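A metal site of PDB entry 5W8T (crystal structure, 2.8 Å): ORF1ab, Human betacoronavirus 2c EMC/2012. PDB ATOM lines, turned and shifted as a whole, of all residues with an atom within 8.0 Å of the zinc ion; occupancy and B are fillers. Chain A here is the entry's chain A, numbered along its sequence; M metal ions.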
ATOM      1  N   TRP A 190      14.169  12.346 -16.995  1.00  0.00           N
ATOM      2  CA  TRP A 190      14.032  13.778 -17.214  1.00  0.00           C
ATOM      3  C   TRP A 190      13.387  14.048 -18.575  1.00  0.00           C
ATOM      4  O   TRP A 190      13.403  13.194 -19.471  1.00  0.00           O
ATOM      5  CB  TRP A 190      15.378  14.513 -17.078  1.00  0.00           C
ATOM      6  CG  TRP A 190      16.431  14.195 -18.102  1.00  0.00           C
ATOM      7  CD1 TRP A 190      16.700  14.893 -19.243  1.00  0.00           C
ATOM      8  CD2 TRP A 190      17.374  13.118 -18.055  1.00  0.00           C
ATOM      9  NE1 TRP A 190      17.753  14.308 -19.922  1.00  0.00           N
ATOM     10  CE2 TRP A 190      18.178  13.218 -19.215  1.00  0.00           C
ATOM     11  CE3 TRP A 190      17.610  12.077 -17.161  1.00  0.00           C
ATOM     12  CZ2 TRP A 190      19.196  12.310 -19.496  1.00  0.00           C
ATOM     13  CZ3 TRP A 190      18.628  11.179 -17.441  1.00  0.00           C
ATOM     14  CH2 TRP A 190      19.412  11.300 -18.596  1.00  0.00           C
ATOM     15  N   CYS A 191      12.766  15.223 -18.679  1.00  0.00           N
ATOM     16  CA  CYS A 191      12.142  15.695 -19.896  1.00  0.00           C
ATOM     17  C   CYS A 191      12.288  17.205 -19.928  1.00  0.00           C
ATOM     18  O   CYS A 191      11.959  17.876 -18.948  1.00  0.00           O
ATOM     19  CB  CYS A 191      10.669  15.302 -19.958  1.00  0.00           C
ATOM     20  SG  CYS A 191       9.659  16.365 -21.027  1.00  0.00           S
ATOM     21  N   ASN A 192      12.772  17.737 -21.062  1.00  0.00           N
ATOM     22  CA  ASN A 192      13.037  19.167 -21.154  1.00  0.00           C
ATOM     23  C   ASN A 192      11.814  20.022 -20.839  1.00  0.00           C
ATOM     24  O   ASN A 192      11.965  21.202 -20.503  1.00  0.00           O
ATOM     25  CB  ASN A 192      13.563  19.538 -22.553  1.00  0.00           C
ATOM     26  CG  ASN A 192      14.948  18.961 -22.833  1.00  0.00           C
ATOM     27  OD1 ASN A 192      15.605  18.428 -21.943  1.00  0.00           O
ATOM     28  ND2 ASN A 192      15.389  19.095 -24.080  1.00  0.00           N
ATOM     29  N   VAL A 193      10.608  19.462 -20.905  1.00  0.00           N
ATOM     30  CA  VAL A 193       9.388  20.191 -20.626  1.00  0.00           C
ATOM     31  C   VAL A 193       8.820  19.855 -19.253  1.00  0.00           C
ATOM     32  O   VAL A 193       8.310  20.738 -18.565  1.00  0.00           O
ATOM     33  CB  VAL A 193       8.347  19.917 -21.736  1.00  0.00           C
ATOM     34  CG1 VAL A 193       7.154  20.858 -21.623  1.00  0.00           C
ATOM     35  CG2 VAL A 193       8.984  20.065 -23.104  1.00  0.00           C
ATOM     36  N   CYS A 194       8.927  18.600 -18.823  1.00  0.00           N
ATOM     37  CA  CYS A 194       8.287  18.137 -17.594  1.00  0.00           C
ATOM     38  C   CYS A 194       9.163  18.263 -16.360  1.00  0.00           C
ATOM     39  O   CYS A 194       8.666  18.619 -15.282  1.00  0.00           O
ATOM     40  CB  CYS A 194       7.855  16.679 -17.749  1.00  0.00           C
ATOM     41  SG  CYS A 194       6.597  16.428 -18.999  1.00  0.00           S
ATOM     42  N   GLY A 195      10.460  17.970 -16.456  1.00  0.00           N
ATOM     43  CA  GLY A 195      11.341  18.119 -15.319  1.00  0.00           C
ATOM     44  C   GLY A 195      12.174  16.875 -15.103  1.00  0.00           C
ATOM     45  O   GLY A 195      12.281  16.014 -15.989  1.00  0.00           O
ATOM     46  N   TYR A 224      12.571   7.651 -24.978  1.00  0.00           N
ATOM     47  CA  TYR A 224      11.259   7.170 -25.374  1.00  0.00           C
ATOM     48  C   TYR A 224      10.270   8.319 -25.254  1.00  0.00           C
ATOM     49  O   TYR A 224      10.587   9.393 -24.733  1.00  0.00           O
ATOM     50  CB  TYR A 224      10.812   5.967 -24.530  1.00  0.00           C
ATOM     51  CG  TYR A 224      10.928   6.199 -23.037  1.00  0.00           C
ATOM     52  CD1 TYR A 224      12.154   6.085 -22.379  1.00  0.00           C
ATOM     53  CD2 TYR A 224       9.807   6.524 -22.272  1.00  0.00           C
ATOM     54  CE1 TYR A 224      12.256   6.294 -21.016  1.00  0.00           C
ATOM     55  CE2 TYR A 224       9.909   6.734 -20.908  1.00  0.00           C
ATOM     56  CZ  TYR A 224      11.135   6.624 -20.286  1.00  0.00           C
ATOM     57  OH  TYR A 224      11.237   6.834 -18.923  1.00  0.00           O
ATOM     58  N   VAL A 225       9.051   8.099 -25.755  1.00  0.00           N
ATOM     59  CA  VAL A 225       8.092   9.200 -25.823  1.00  0.00           C
ATOM     60  C   VAL A 225       7.585   9.535 -24.424  1.00  0.00           C
ATOM     61  O   VAL A 225       7.293   8.639 -23.608  1.00  0.00           O
ATOM     62  CB  VAL A 225       6.931   8.874 -26.774  1.00  0.00           C
ATOM     63  CG1 VAL A 225       6.013   7.807 -26.208  1.00  0.00           C
ATOM     64  CG2 VAL A 225       6.165  10.148 -27.104  1.00  0.00           C
ATOM     65  N   CYS A 226       7.503  10.817 -24.143  1.00  0.00           N
ATOM     66  CA  CYS A 226       7.024  11.326 -22.856  1.00  0.00           C
ATOM     67  C   CYS A 226       5.521  11.573 -22.920  1.00  0.00           C
ATOM     68  O   CYS A 226       4.912  11.620 -23.989  1.00  0.00           O
ATOM     69  CB  CYS A 226       7.762  12.606 -22.490  1.00  0.00           C
ATOM     70  SG  CYS A 226       7.450  13.237 -20.829  1.00  0.00           S
ATOM     71  N   GLN A 227       4.907  11.720 -21.738  1.00  0.00           N
ATOM     72  CA  GLN A 227       3.465  11.898 -21.697  1.00  0.00           C
ATOM     73  C   GLN A 227       3.056  13.244 -22.284  1.00  0.00           C
ATOM     74  O   GLN A 227       1.888  13.416 -22.641  1.00  0.00           O
ATOM     75  CB  GLN A 227       2.960  11.753 -20.261  1.00  0.00           C
ATOM     76  CG  GLN A 227       1.449  11.608 -20.192  1.00  0.00           C
ATOM     77  CD  GLN A 227       0.902  11.609 -18.774  1.00  0.00           C
ATOM     78  OE1 GLN A 227       1.661  11.495 -17.808  1.00  0.00           O
ATOM     79  NE2 GLN A 227      -0.408  11.748 -18.648  1.00  0.00           N
ATOM     80  N   CYS A 228       4.004  14.179 -22.404  1.00  0.00           N
ATOM     81  CA  CYS A 228       3.780  15.484 -23.003  1.00  0.00           C
ATOM     82  C   CYS A 228       3.862  15.457 -24.534  1.00  0.00           C
ATOM     83  O   CYS A 228       3.324  16.364 -25.183  1.00  0.00           O
ATOM     84  CB  CYS A 228       4.815  16.479 -22.461  1.00  0.00           C
ATOM     85  SG  CYS A 228       6.501  16.206 -23.053  1.00  0.00           S
ATOM     86  N   GLY A 229       4.512  14.440 -25.110  1.00  0.00           N
ATOM     87  CA  GLY A 229       4.737  14.350 -26.541  1.00  0.00           C
ATOM     88  C   GLY A 229       6.189  14.441 -26.947  1.00  0.00           C
ATOM     89  O   GLY A 229       6.563  13.940 -28.014  1.00  0.00           O
ATOM     90  N   GLY A 230       7.031  15.067 -26.116  1.00  0.00           N
ATOM     91  CA  GLY A 230       8.457  15.137 -26.348  1.00  0.00           C
ATOM     92  C   GLY A 230       9.136  13.792 -26.130  1.00  0.00           C
ATOM     93  O   GLY A 230       8.489  12.747 -26.016  1.00  0.00           O
ATOM     94  N   GLU A 231      10.468  13.828 -26.058  1.00  0.00           N
ATOM     95  CA  GLU A 231      11.220  12.617 -25.744  1.00  0.00           C
ATOM     96  C   GLU A 231      11.737  12.690 -24.309  1.00  0.00           C
ATOM     97  O   GLU A 231      12.518  13.585 -23.966  1.00  0.00           O
ATOM     98  CB  GLU A 231      12.362  12.319 -26.727  1.00  0.00           C
ATOM     99  CG  GLU A 231      13.000  13.447 -27.471  1.00  0.00           C
ATOM    100  CD  GLU A 231      14.050  12.922 -28.455  1.00  0.00           C
ATOM    101  OE1 GLU A 231      14.123  11.705 -28.693  1.00  0.00           O
ATOM    102  OE2 GLU A 231      14.782  13.719 -29.038  1.00  0.00           O
ATOM    103  N   ARG A 232      11.260  11.763 -23.482  1.00  0.00           N
ATOM    104  CA  ARG A 232      11.749  11.596 -22.131  1.00  0.00           C
ATOM    105  C   ARG A 232      13.020  10.748 -22.146  1.00  0.00           C
ATOM    106  O   ARG A 232      13.186   9.847 -22.982  1.00  0.00           O
ATOM    107  CB  ARG A 232      10.673  10.943 -21.249  1.00  0.00           C
ATOM    108  CG  ARG A 232      11.037  10.748 -19.781  1.00  0.00           C
ATOM    109  CD  ARG A 232       9.804  10.492 -18.918  1.00  0.00           C
ATOM    110  NE  ARG A 232       8.867   9.565 -19.563  1.00  0.00           N
ATOM    111  CZ  ARG A 232       7.780   9.055 -18.992  1.00  0.00           C
ATOM    112  NH1 ARG A 232       7.464   9.366 -17.740  1.00  0.00           N
ATOM    113  NH2 ARG A 232       7.000   8.223 -19.668  1.00  0.00           N
ATOM    114  N   HIS A 233      13.915  11.044 -21.214  1.00  0.00           N
ATOM    115  CA  HIS A 233      15.152  10.310 -21.077  1.00  0.00           C
ATOM    116  C   HIS A 233      15.169   9.598 -19.730  1.00  0.00           C
ATOM    117  O   HIS A 233      14.499  10.012 -18.781  1.00  0.00           O
ATOM    118  CB  HIS A 233      16.345  11.244 -21.230  1.00  0.00           C
ATOM    119  CG  HIS A 233      16.352  11.981 -22.540  1.00  0.00           C
ATOM    120  ND1 HIS A 233      16.746  11.383 -23.724  1.00  0.00           N
ATOM    121  CD2 HIS A 233      16.000  13.247 -22.850  1.00  0.00           C
ATOM    122  CE1 HIS A 233      16.635  12.266 -24.707  1.00  0.00           C
ATOM    123  NE2 HIS A 233      16.196  13.401 -24.207  1.00  0.00           N
HETATM  124 ZN    ZN M   1       7.430  15.582 -21.129  1.00  0.00          ZN
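SG of Cys 228 sits close to N of Gly 230 (3.3 Å). SG of Cys 191 sits close to N of Val 193, at 3.2 Å.
The zinc ion is bound by the side-chain sulfur (SG) of Cys 228 (2.2 Å). The zinc ion is bound by SG of Cys 226 (2.4 Å). The side-chain sulfur (SG) of Cys 191 is bound to the zinc ion (2.4 Å). SG of Cys 194 is bound to the zinc ion (2.4 Å).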
